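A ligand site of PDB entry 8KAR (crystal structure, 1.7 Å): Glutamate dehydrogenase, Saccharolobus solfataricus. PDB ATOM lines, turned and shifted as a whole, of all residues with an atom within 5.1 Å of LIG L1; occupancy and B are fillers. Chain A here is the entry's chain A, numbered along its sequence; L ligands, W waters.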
ATOM      1  N   ARG A  76      10.713  -1.802  32.620  1.00  0.00           N
ATOM      2  CA  ARG A  76      11.139  -1.402  31.239  1.00  0.00           C
ATOM      3  C   ARG A  76      11.279   0.061  31.060  1.00  0.00           C
ATOM      4  O   ARG A  76      10.543   0.840  31.633  1.00  0.00           O
ATOM      5  CB  ARG A  76      10.165  -1.921  30.169  1.00  0.00           C
ATOM      6  CG  ARG A  76       8.697  -1.589  30.363  1.00  0.00           C
ATOM      7  CD  ARG A  76       7.894  -1.980  29.123  1.00  0.00           C
ATOM      8  NE  ARG A  76       8.083  -3.386  28.766  1.00  0.00           N
ATOM      9  CZ  ARG A  76       7.552  -3.999  27.726  1.00  0.00           C
ATOM     10  NH1 ARG A  76       6.786  -3.332  26.872  1.00  0.00           N
ATOM     11  NH2 ARG A  76       7.799  -5.286  27.516  1.00  0.00           N
ATOM     12  N   LEU A  89       1.147  -5.426  31.569  1.00  0.00           N
ATOM     13  CA  LEU A  89       2.297  -6.282  31.780  1.00  0.00           C
ATOM     14  C   LEU A  89       2.260  -6.911  33.174  1.00  0.00           C
ATOM     15  O   LEU A  89       2.604  -8.084  33.289  1.00  0.00           O
ATOM     16  CB  LEU A  89       3.578  -5.500  31.544  1.00  0.00           C
ATOM     17  CG  LEU A  89       3.855  -5.092  30.119  1.00  0.00           C
ATOM     18  CD1 LEU A  89       4.977  -4.074  30.065  1.00  0.00           C
ATOM     19  CD2 LEU A  89       4.233  -6.350  29.299  1.00  0.00           C
ATOM     20  N   LYS A  96       1.549 -15.812  34.758  1.00  0.00           N
ATOM     21  CA  LYS A  96       2.785 -16.567  34.568  1.00  0.00           C
ATOM     22  C   LYS A  96       3.225 -17.191  35.887  1.00  0.00           C
ATOM     23  O   LYS A  96       3.587 -18.365  35.929  1.00  0.00           O
ATOM     24  CB  LYS A  96       3.789 -15.566  33.934  1.00  0.00           C
ATOM     25  CG  LYS A  96       5.269 -15.870  33.975  1.00  0.00           C
ATOM     26  CD  LYS A  96       6.195 -14.863  33.275  1.00  0.00           C
ATOM     27  CE  LYS A  96       5.526 -13.934  32.286  1.00  0.00           C
ATOM     28  NZ  LYS A  96       6.531 -13.180  31.477  1.00  0.00           N
ATOM     29  N   LYS A 108       4.902  -5.025  37.818  1.00  0.00           N
ATOM     30  CA  LYS A 108       5.684  -4.550  36.682  1.00  0.00           C
ATOM     31  C   LYS A 108       5.965  -3.066  36.838  1.00  0.00           C
ATOM     32  O   LYS A 108       5.209  -2.306  37.440  1.00  0.00           O
ATOM     33  CB  LYS A 108       4.908  -4.858  35.404  1.00  0.00           C
ATOM     34  CG  LYS A 108       5.573  -4.527  34.091  1.00  0.00           C
ATOM     35  CD  LYS A 108       6.790  -5.232  33.809  1.00  0.00           C
ATOM     36  CE  LYS A 108       6.643  -6.719  33.787  1.00  0.00           C
ATOM     37  NZ  LYS A 108       7.538  -7.253  32.737  1.00  0.00           N
ATOM     38  N   PRO A 147      14.904  -7.018  35.499  1.00  0.00           N
ATOM     39  CA  PRO A 147      14.996  -6.387  34.172  1.00  0.00           C
ATOM     40  C   PRO A 147      13.778  -6.604  33.253  1.00  0.00           C
ATOM     41  O   PRO A 147      12.893  -7.435  33.514  1.00  0.00           O
ATOM     42  CB  PRO A 147      16.147  -7.150  33.514  1.00  0.00           C
ATOM     43  CG  PRO A 147      16.994  -7.639  34.681  1.00  0.00           C
ATOM     44  CD  PRO A 147      15.930  -8.083  35.666  1.00  0.00           C
ATOM     45  N   ASP A 148      13.751  -5.843  32.163  1.00  0.00           N
ATOM     46  CA  ASP A 148      12.811  -6.016  31.080  1.00  0.00           C
ATOM     47  C   ASP A 148      13.405  -5.214  29.942  1.00  0.00           C
ATOM     48  O   ASP A 148      14.622  -5.115  29.895  1.00  0.00           O
ATOM     49  CB  ASP A 148      11.382  -5.620  31.454  1.00  0.00           C
ATOM     50  CG  ASP A 148      10.343  -6.161  30.491  1.00  0.00           C
ATOM     51  OD1 ASP A 148       9.893  -7.352  30.698  1.00  0.00           O
ATOM     52  OD2 ASP A 148       9.898  -5.364  29.574  1.00  0.00           O
ATOM     53  N   ILE A 149      12.595  -4.673  29.015  1.00  0.00           N
ATOM     54  CA  ILE A 149      13.219  -3.968  27.891  1.00  0.00           C
ATOM     55  C   ILE A 149      14.044  -2.794  28.395  1.00  0.00           C
ATOM     56  O   ILE A 149      13.528  -1.940  29.104  1.00  0.00           O
ATOM     57  CB  ILE A 149      12.150  -3.473  26.890  1.00  0.00           C
ATOM     58  CG1 ILE A 149      11.362  -4.650  26.299  1.00  0.00           C
ATOM     59  CG2 ILE A 149      12.819  -2.650  25.792  1.00  0.00           C
ATOM     60  CD1 ILE A 149      10.243  -4.230  25.338  1.00  0.00           C
ATOM     61  N   ASN A 150      15.286  -2.689  27.856  1.00  0.00           N
ATOM     62  CA  ASN A 150      16.221  -1.614  28.110  1.00  0.00           C
ATOM     63  C   ASN A 150      16.730  -1.571  29.553  1.00  0.00           C
ATOM     64  O   ASN A 150      17.379  -0.595  29.943  1.00  0.00           O
ATOM     65  CB  ASN A 150      15.651  -0.281  27.608  1.00  0.00           C
ATOM     66  CG  ASN A 150      15.832  -0.056  26.120  1.00  0.00           C
ATOM     67  OD1 ASN A 150      16.834  -0.447  25.530  1.00  0.00           O
ATOM     68  ND2 ASN A 150      14.815   0.504  25.462  1.00  0.00           N
ATOM     69  N   THR A 151      16.489  -2.593  30.380  1.00  0.00           N
ATOM     70  CA  THR A 151      17.181  -2.678  31.660  1.00  0.00           C
ATOM     71  C   THR A 151      17.895  -4.029  31.696  1.00  0.00           C
ATOM     72  O   THR A 151      17.616  -4.883  30.885  1.00  0.00           O
ATOM     73  CB  THR A 151      16.266  -2.422  32.848  1.00  0.00           C
ATOM     74  OG1 THR A 151      15.295  -3.466  32.895  1.00  0.00           O
ATOM     75  CG2 THR A 151      15.575  -1.070  32.773  1.00  0.00           C
ATOM     76  N   ARG A 188      20.818 -16.729  35.069  1.00  0.00           N
ATOM     77  CA  ARG A 188      19.718 -15.779  34.886  1.00  0.00           C
ATOM     78  C   ARG A 188      19.894 -14.880  33.655  1.00  0.00           C
ATOM     79  O   ARG A 188      18.925 -14.430  33.057  1.00  0.00           O
ATOM     80  CB  ARG A 188      19.515 -14.930  36.132  1.00  0.00           C
ATOM     81  CG  ARG A 188      18.394 -13.903  36.054  1.00  0.00           C
ATOM     82  CD  ARG A 188      17.073 -14.545  35.672  1.00  0.00           C
ATOM     83  NE  ARG A 188      15.979 -13.599  35.560  1.00  0.00           N
ATOM     84  CZ  ARG A 188      15.671 -12.943  34.452  1.00  0.00           C
ATOM     85  NH1 ARG A 188      16.408 -13.113  33.362  1.00  0.00           N
ATOM     86  NH2 ARG A 188      14.631 -12.112  34.428  1.00  0.00           N
ATOM     87  N   THR A 192      15.819 -16.717  30.212  1.00  0.00           N
ATOM     88  CA  THR A 192      14.613 -16.550  29.413  1.00  0.00           C
ATOM     89  C   THR A 192      14.768 -17.261  28.057  1.00  0.00           C
ATOM     90  O   THR A 192      13.887 -18.017  27.620  1.00  0.00           O
ATOM     91  CB  THR A 192      14.237 -15.090  29.214  1.00  0.00           C
ATOM     92  OG1 THR A 192      14.263 -14.443  30.476  1.00  0.00           O
ATOM     93  CG2 THR A 192      12.881 -14.965  28.560  1.00  0.00           C
ATOM     94  N   GLN A 219      11.671 -12.154  16.188  1.00  0.00           N
ATOM     95  CA  GLN A 219      11.538 -10.704  16.196  1.00  0.00           C
ATOM     96  C   GLN A 219      12.120 -10.161  17.490  1.00  0.00           C
ATOM     97  O   GLN A 219      11.709 -10.584  18.549  1.00  0.00           O
ATOM     98  CB  GLN A 219      10.106 -10.230  16.009  1.00  0.00           C
ATOM     99  CG  GLN A 219      10.002  -8.714  16.011  1.00  0.00           C
ATOM    100  CD  GLN A 219       8.585  -8.201  16.040  1.00  0.00           C
ATOM    101  OE1 GLN A 219       7.766  -8.678  16.829  1.00  0.00           O
ATOM    102  NE2 GLN A 219       8.316  -7.261  15.133  1.00  0.00           N
ATOM    103  N   GLY A 220      13.158  -9.315  17.376  1.00  0.00           N
ATOM    104  CA  GLY A 220      13.891  -8.864  18.536  1.00  0.00           C
ATOM    105  C   GLY A 220      15.168  -9.651  18.715  1.00  0.00           C
ATOM    106  O   GLY A 220      15.229 -10.820  18.340  1.00  0.00           O
ATOM    107  N   PHE A 221      16.222  -8.948  19.156  1.00  0.00           N
ATOM    108  CA  PHE A 221      17.527  -9.585  19.259  1.00  0.00           C
ATOM    109  C   PHE A 221      18.276  -9.110  20.502  1.00  0.00           C
ATOM    110  O   PHE A 221      19.498  -8.978  20.479  1.00  0.00           O
ATOM    111  CB  PHE A 221      18.331  -9.280  17.999  1.00  0.00           C
ATOM    112  CG  PHE A 221      19.349 -10.320  17.635  1.00  0.00           C
ATOM    113  CD1 PHE A 221      18.946 -11.598  17.277  1.00  0.00           C
ATOM    114  CD2 PHE A 221      20.696 -10.007  17.584  1.00  0.00           C
ATOM    115  CE1 PHE A 221      19.890 -12.552  16.931  1.00  0.00           C
ATOM    116  CE2 PHE A 221      21.629 -10.961  17.216  1.00  0.00           C
ATOM    117  CZ  PHE A 221      21.224 -12.222  16.867  1.00  0.00           C
ATOM    118  N   GLY A 222      17.553  -8.840  21.584  1.00  0.00           N
ATOM    119  CA  GLY A 222      18.219  -8.498  22.820  1.00  0.00           C
ATOM    120  C   GLY A 222      18.352  -9.697  23.768  1.00  0.00           C
ATOM    121  O   GLY A 222      18.648 -10.842  23.380  1.00  0.00           O
ATOM    122  N   ASN A 223      18.074  -9.424  25.014  1.00  0.00           N
ATOM    123  CA  ASN A 223      18.289 -10.462  26.041  1.00  0.00           C
ATOM    124  C   ASN A 223      17.533 -11.757  25.701  1.00  0.00           C
ATOM    125  O   ASN A 223      18.116 -12.843  25.693  1.00  0.00           O
ATOM    126  CB  ASN A 223      17.908  -9.997  27.437  1.00  0.00           C
ATOM    127  CG  ASN A 223      18.265 -11.059  28.452  1.00  0.00           C
ATOM    128  OD1 ASN A 223      17.392 -11.729  29.021  1.00  0.00           O
ATOM    129  ND2 ASN A 223      19.573 -11.224  28.643  1.00  0.00           N
ATOM    130  N   VAL A 224      16.240 -11.654  25.340  1.00  0.00           N
ATOM    131  CA  VAL A 224      15.446 -12.819  24.989  1.00  0.00           C
ATOM    132  C   VAL A 224      15.812 -13.317  23.587  1.00  0.00           C
ATOM    133  O   VAL A 224      16.116 -14.514  23.393  1.00  0.00           O
ATOM    134  CB  VAL A 224      13.931 -12.530  25.148  1.00  0.00           C
ATOM    135  CG1 VAL A 224      13.086 -13.752  24.805  1.00  0.00           C
ATOM    136  CG2 VAL A 224      13.583 -12.015  26.545  1.00  0.00           C
ATOM    137  N   GLY A 225      15.758 -12.420  22.595  1.00  0.00           N
ATOM    138  CA  GLY A 225      15.910 -12.807  21.199  1.00  0.00           C
ATOM    139  C   GLY A 225      17.289 -13.363  20.852  1.00  0.00           C
ATOM    140  O   GLY A 225      17.386 -14.381  20.142  1.00  0.00           O
ATOM    141  N   SER A 243      15.365  -9.731  13.817  1.00  0.00           N
ATOM    142  CA  SER A 243      15.115  -8.300  13.675  1.00  0.00           C
ATOM    143  C   SER A 243      15.325  -7.600  15.003  1.00  0.00           C
ATOM    144  O   SER A 243      15.408  -8.241  16.059  1.00  0.00           O
ATOM    145  CB  SER A 243      13.688  -8.021  13.182  1.00  0.00           C
ATOM    146  OG  SER A 243      12.749  -8.189  14.256  1.00  0.00           O
ATOM    147  N   ASP A 244      15.353  -6.269  14.909  1.00  0.00           N
ATOM    148  CA  ASP A 244      15.324  -5.403  16.081  1.00  0.00           C
ATOM    149  C   ASP A 244      14.633  -4.106  15.678  1.00  0.00           C
ATOM    150  O   ASP A 244      13.977  -4.056  14.650  1.00  0.00           O
ATOM    151  CB  ASP A 244      16.729  -5.291  16.716  1.00  0.00           C
ATOM    152  CG  ASP A 244      17.807  -4.633  15.867  1.00  0.00           C
ATOM    153  OD1 ASP A 244      17.467  -3.930  14.894  1.00  0.00           O
ATOM    154  OD2 ASP A 244      18.993  -4.824  16.178  1.00  0.00           O
ATOM    155  N   ILE A 245      14.729  -3.066  16.510  1.00  0.00           N
ATOM    156  CA  ILE A 245      14.019  -1.815  16.245  1.00  0.00           C
ATOM    157  C   ILE A 245      14.479  -1.173  14.934  1.00  0.00           C
ATOM    158  O   ILE A 245      13.728  -0.427  14.309  1.00  0.00           O
ATOM    159  CB  ILE A 245      14.240  -0.864  17.440  1.00  0.00           C
ATOM    160  CG1 ILE A 245      13.349   0.383  17.349  1.00  0.00           C
ATOM    161  CG2 ILE A 245      15.692  -0.455  17.567  1.00  0.00           C
ATOM    162  CD1 ILE A 245      12.030   0.272  17.982  1.00  0.00           C
ATOM    163  N   ASN A 281       9.960  -4.958   9.929  1.00  0.00           N
ATOM    164  CA  ASN A 281       9.471  -5.845  10.975  1.00  0.00           C
ATOM    165  C   ASN A 281       8.122  -6.435  10.579  1.00  0.00           C
ATOM    166  O   ASN A 281       7.820  -7.606  10.863  1.00  0.00           O
ATOM    167  CB  ASN A 281       9.402  -5.103  12.314  1.00  0.00           C
ATOM    168  CG  ASN A 281      10.642  -5.297  13.147  1.00  0.00           C
ATOM    169  OD1 ASN A 281      10.811  -6.374  13.727  1.00  0.00           O
ATOM    170  ND2 ASN A 281      11.474  -4.267  13.257  1.00  0.00           N
ATOM    171  N   ALA A 295       9.874 -11.729  20.015  1.00  0.00           N
ATOM    172  CA  ALA A 295      10.731 -11.586  21.172  1.00  0.00           C
ATOM    173  C   ALA A 295      11.065 -10.112  21.457  1.00  0.00           C
ATOM    174  O   ALA A 295      12.155  -9.847  21.984  1.00  0.00           O
ATOM    175  CB  ALA A 295      12.013 -12.357  21.018  1.00  0.00           C
ATOM    176  N   ALA A 296      10.168  -9.195  21.090  1.00  0.00           N
ATOM    177  CA  ALA A 296      10.490  -7.770  21.195  1.00  0.00           C
ATOM    178  C   ALA A 296       9.455  -7.055  22.043  1.00  0.00           C
ATOM    179  O   ALA A 296       9.715  -6.817  23.216  1.00  0.00           O
ATOM    180  CB  ALA A 296      10.637  -7.135  19.813  1.00  0.00           C
ATOM    181  N   VAL A 297       8.318  -6.692  21.421  1.00  0.00           N
ATOM    182  CA  VAL A 297       7.280  -5.912  22.074  1.00  0.00           C
ATOM    183  C   VAL A 297       5.920  -6.591  21.890  1.00  0.00           C
ATOM    184  O   VAL A 297       5.774  -7.640  21.225  1.00  0.00           O
ATOM    185  CB  VAL A 297       7.280  -4.432  21.613  1.00  0.00           C
ATOM    186  CG1 VAL A 297       8.586  -3.708  21.968  1.00  0.00           C
ATOM    187  CG2 VAL A 297       6.964  -4.279  20.129  1.00  0.00           C
ATOM    188  N   GLY A 317       8.148 -15.271  23.058  1.00  0.00           N
ATOM    189  CA  GLY A 317       9.218 -14.853  23.962  1.00  0.00           C
ATOM    190  C   GLY A 317       8.893 -13.496  24.580  1.00  0.00           C
ATOM    191  O   GLY A 317       9.059 -13.315  25.773  1.00  0.00           O
ATOM    192  N   ALA A 318       8.343 -12.585  23.787  1.00  0.00           N
ATOM    193  CA  ALA A 318       7.818 -11.305  24.297  1.00  0.00           C
ATOM    194  C   ALA A 318       6.597 -11.529  25.189  1.00  0.00           C
ATOM    195  O   ALA A 318       5.898 -12.532  25.080  1.00  0.00           O
ATOM    196  CB  ALA A 318       7.426 -10.466  23.097  1.00  0.00           C
ATOM    197  N   ASN A 319       6.261 -10.548  26.038  1.00  0.00           N
ATOM    198  CA  ASN A 319       4.991 -10.509  26.722  1.00  0.00           C
ATOM    199  C   ASN A 319       3.931  -9.881  25.815  1.00  0.00           C
ATOM    200  O   ASN A 319       4.142  -8.782  25.254  1.00  0.00           O
ATOM    201  CB  ASN A 319       5.118  -9.692  28.013  1.00  0.00           C
ATOM    202  CG  ASN A 319       5.951 -10.423  29.053  1.00  0.00           C
ATOM    203  OD1 ASN A 319       5.471 -11.414  29.593  1.00  0.00           O
ATOM    204  ND2 ASN A 319       7.158  -9.953  29.367  1.00  0.00           N
ATOM    205  N   ASN A 344       7.944 -17.911  28.072  1.00  0.00           N
ATOM    206  CA  ASN A 344       8.955 -16.921  28.449  1.00  0.00           C
ATOM    207  C   ASN A 344       9.323 -16.969  29.941  1.00  0.00           C
ATOM    208  O   ASN A 344      10.139 -16.158  30.410  1.00  0.00           O
ATOM    209  CB  ASN A 344       8.607 -15.519  27.913  1.00  0.00           C
ATOM    210  CG  ASN A 344       7.583 -14.727  28.708  1.00  0.00           C
ATOM    211  OD1 ASN A 344       7.328 -15.018  29.892  1.00  0.00           O
ATOM    212  ND2 ASN A 344       6.896 -13.798  28.039  1.00  0.00           N
ATOM    213  N   GLY A 347      12.667 -16.495  32.503  1.00  0.00           N
ATOM    214  CA  GLY A 347      13.083 -15.275  33.166  1.00  0.00           C
ATOM    215  C   GLY A 347      12.749 -15.304  34.646  1.00  0.00           C
ATOM    216  O   GLY A 347      13.648 -15.322  35.506  1.00  0.00           O
HETATM  217  P1  LIG L   1      16.023  -5.964  25.413  1.00  0.00           P
HETATM  218  O1  LIG L   1      15.884  -4.503  25.745  1.00  0.00           O
HETATM  219  O2  LIG L   1      17.241  -6.733  25.909  1.00  0.00           O
HETATM  220  O3  LIG L   1      15.819  -6.207  23.874  1.00  0.00           O
HETATM  221  C1  LIG L   1      14.776  -5.632  23.125  1.00  0.00           C
HETATM  222  C2  LIG L   1      14.977  -6.012  21.685  1.00  0.00           C
HETATM  223  O4  LIG L   1      13.750  -5.741  20.982  1.00  0.00           O
HETATM  224  C3  LIG L   1      16.073  -5.271  20.917  1.00  0.00           C
HETATM  225  O5  LIG L   1      16.554  -6.224  19.967  1.00  0.00           O
HETATM  226  C4  LIG L   1      15.297  -4.080  20.357  1.00  0.00           C
HETATM  227  O6  LIG L   1      15.937  -3.418  19.271  1.00  0.00           O
HETATM  228  C5  LIG L   1      14.028  -4.816  19.951  1.00  0.00           C
HETATM  229  N1  LIG L   1      12.860  -3.977  19.744  1.00  0.00           N
HETATM  230  C6  LIG L   1      12.476  -2.886  20.493  1.00  0.00           C
HETATM  231  N2  LIG L   1      11.428  -2.280  20.010  1.00  0.00           N
HETATM  232  C7  LIG L   1      11.121  -2.993  18.868  1.00  0.00           C
HETATM  233  C8  LIG L   1      10.104  -2.843  17.914  1.00  0.00           C
HETATM  234  N3  LIG L   1       9.185  -1.902  18.006  1.00  0.00           N
HETATM  235  N4  LIG L   1      10.064  -3.717  16.883  1.00  0.00           N
HETATM  236  C9  LIG L   1      11.016  -4.656  16.816  1.00  0.00           C
HETATM  237  N5  LIG L   1      12.009  -4.894  17.654  1.00  0.00           N
HETATM  238  C10 LIG L   1      12.021  -4.008  18.659  1.00  0.00           C
HETATM  239  O7  LIG L   1      14.674  -6.629  26.038  1.00  0.00           O
HETATM  240  P2  LIG L   1      14.345  -8.151  26.322  1.00  0.00           P
HETATM  241  O8  LIG L   1      14.762  -8.451  27.740  1.00  0.00           O
HETATM  242  O9  LIG L   1      14.900  -9.035  25.248  1.00  0.00           O
HETATM  243  O10 LIG L   1      12.754  -8.198  26.264  1.00  0.00           O
HETATM  244  C11 LIG L   1      12.054  -8.533  25.008  1.00  0.00           C
HETATM  245  C12 LIG L   1      10.666  -9.039  25.307  1.00  0.00           C
HETATM  246  O11 LIG L   1      10.729 -10.178  26.216  1.00  0.00           O
HETATM  247  C13 LIG L   1       9.718  -8.043  25.984  1.00  0.00           C
HETATM  248  O12 LIG L   1       8.326  -8.281  25.733  1.00  0.00           O
HETATM  249  C14 LIG L   1       9.898  -8.417  27.463  1.00  0.00           C
HETATM  250  O13 LIG L   1       8.820  -8.059  28.338  1.00  0.00           O
HETATM  251  C15 LIG L   1       9.885  -9.952  27.309  1.00  0.00           C
HETATM  252  N6  LIG L   1      10.470 -10.719  28.443  1.00  0.00           N
HETATM  253  C16 LIG L   1      11.703 -10.389  28.947  1.00  0.00           C
HETATM  254  C17 LIG L   1      12.204 -11.118  30.018  1.00  0.00           C
HETATM  255  C18 LIG L   1      13.543 -10.894  30.625  1.00  0.00           C
HETATM  256  O14 LIG L   1      13.926 -11.757  31.441  1.00  0.00           O
HETATM  257  N7  LIG L   1      14.352  -9.976  30.076  1.00  0.00           N
HETATM  258  C19 LIG L   1      11.479 -12.189  30.526  1.00  0.00           C
HETATM  259  C20 LIG L   1      10.268 -12.536  29.957  1.00  0.00           C
HETATM  260  C21 LIG L   1       9.808 -11.818  28.893  1.00  0.00           C
HETATM  261  C1  LG2 L   2       8.919 -11.098  32.694  1.00  0.00           C
HETATM  262  O1  LG2 L   2       8.748 -12.292  32.903  1.00  0.00           O
HETATM  263  O2  LG2 L   2       8.451 -10.522  31.714  1.00  0.00           O
HETATM  264  C2  LG2 L   2       9.614 -10.429  33.568  1.00  0.00           C
HETATM  265  O3  LG2 L   2       9.267  -9.302  33.895  1.00  0.00           O
HETATM  266  C3  LG2 L   2      10.819 -11.019  34.255  1.00  0.00           C
HETATM  267  C4  LG2 L   2      10.861 -10.521  35.680  1.00  0.00           C
HETATM  268  C5  LG2 L   2      11.549 -11.451  36.655  1.00  0.00           C
HETATM  269  O4  LG2 L   2      12.493 -12.147  36.241  1.00  0.00           O
HETATM  270  O5  LG2 L   2      11.125 -11.484  37.819  1.00  0.00           O
HETATM  271  O   HOH W   1      14.451  -1.275  22.569  1.00  0.00           O
HETATM  272  O   HOH W   2      14.769  -9.624  22.589  1.00  0.00           O
HETATM  273  O   HOH W   3       5.950  -6.822  25.718  1.00  0.00           O
HETATM  274  O   HOH W   4      16.628  -2.552  24.007  1.00  0.00           O
HETATM  275  O   HOH W   5      18.997  -5.330  18.862  1.00  0.00           O
HETATM  276  O   HOH W   6       8.351  -3.689  15.011  1.00  0.00           O
HETATM  277  O   HOH W   7      16.355  -7.381  29.733  1.00  0.00           O
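OD1 of Asp 148 is in hydrogen-bond range of O13 of LIG L1. N of Asn 319 is in hydrogen-bond range of O12 of LIG L1 (3.1 Å). O13 of LIG L1 lies within hydrogen-bond range of ND2 of Asn 319. An oxygen (O1) of LIG L1 is in hydrogen-bond range of the backbone NH (N) of Asn 150 (2.8 Å). The backbone NH (N) of Phe 221 is in hydrogen-bond range of an oxygen (O5) of LIG L1, 2.9 Å away. The side-chain hydroxyl (OG1) of Thr 192 lies within hydrogen-bond range of an oxygen (O14) of LIG L1, 2.9 Å away. The backbone NH (N) of Val 224 is in hydrogen-bond range of an oxygen (O9) of LIG L1 (2.9 Å). The backbone NH of Asn 223 lies within hydrogen-bond range of an oxygen (O2) of LIG L1 (3.0 Å). An oxygen (O12) of LIG L1 lies close to the backbone carbonyl oxygen of Ala 296, at 3.2 Å. The backbone NH of Ile 245 sits at hydrogen-bond distance from an oxygen (O6) of LIG L1 (3.0 Å). The guanidinium group (NH2) of Arg 76 sits at hydrogen-bond distance from an oxygen (O13) of LIG L1. NH2 of Arg 188 lies within hydrogen-bond range of O14 of LIG L1. O5 of LIG L1 is in hydrogen-bond range of N of Gly 222. An oxygen (O2) of LG2 L2 sits at hydrogen-bond distance from the side-chain amide nitrogen of Asn 319 (2.7 Å). An oxygen (O4) of LG2 L2 is in salt-bridge range of the guanidinium group (NH2) of Arg 188 (2.8 Å). The side-chain amino group (NZ) of Lys 96 lies within salt-bridge range of an oxygen (O1) of LG2 L2, at 2.8 Å. The side-chain amino group (NZ) of Lys 108 lies within salt-bridge range of an oxygen (O2) of LG2 L2, 3.5 Å away.
The backbone NH of Asp 148 lies within hydrogen-bond range of the side-chain hydroxyl of Thr 151. The side-chain amide oxygen of Asn 319 lies within hydrogen-bond range of the side-chain amide nitrogen of Asn 344 (3.2 Å). OD1 of Asn 319 is in hydrogen-bond range of NZ of Lys 96, 2.8 Å away. The backbone carbonyl oxygen of Ser 243 lies within hydrogen-bond range of the backbone NH of Phe 221 (3.3 Å). The backbone NH of Ala 296 sits at hydrogen-bond distance from the backbone carbonyl oxygen of Gln 219, at 3.3 Å. The side-chain amide nitrogen (ND2) of Asn 344 sits at hydrogen-bond distance from the backbone carbonyl oxygen (O) of Ala 318 (3.4 Å). OD1 of Asn 281 is in hydrogen-bond range of OG of Ser 243 (2.7 Å). O of Ser 243 is in hydrogen-bond range of N of Gly 220 (2.8 Å).
Water W4 bridges the side-chain amide oxygen (OD1) of Asn 150 (2.6 Å) and an oxygen (O1) of LIG L1 (2.7 Å). Water W2 lies within hydrogen-bond range of O of Ala 295 (2.7 Å), O9 of LIG L1 (2.7 Å), N of Gly 225 (3.0 Å) and N of Gly 222 (3.1 Å). Water W7 lies within hydrogen-bond range of O8 of LIG L1 (2.8 Å), O of Asp 148 (2.9 Å) and O of Thr 151 (3.0 Å). Water W3 lies within hydrogen-bond range of the backbone carbonyl oxygen of Asn 319 (2.7 Å), an oxygen (O12) of LIG L1 (2.8 Å) and the guanidinium group of Arg 76 (3.0 Å). Water W5 lies within hydrogen-bond range of OD2 of Asp 244 (2.7 Å) and O5 of LIG L1 (2.8 Å).
Merely in contact with LIG L1: Ile 149 (3.5 Å), Gly 220 (3.9 Å), Asp 244 (3.3 Å), Asn 281 (3.5 Å), Ala 295 (3.3 Å), Val 297 (3.7 Å), Gly 317 (3.5 Å), Ala 318 (3.4 Å) and Asn 344 (3.6 Å). Hydrophobic or aromatic side chains within 4 Å of LIG L1: Ile 149, Val 224, Ile 245, Ala 296, Val 297 and Ala 318. Within 4 Å of LIG L1: Arg 76, Asp 148, Ile 149, Asn 150, Arg 188, Thr 192, Gly 220, Phe 221, Gly 222, Asn 223, Val 224, Asp 244, Ile 245, Asn 281, Ala 295, Ala 296, Val 297, Gly 317, Ala 318, Asn 319 and Asn 344. Along chain A the residues within 4 Å of LIG L1 span positions 76 to 344. The nearest printed residue that does not touch LIG L1 is Gly 347 (4.01 Å).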
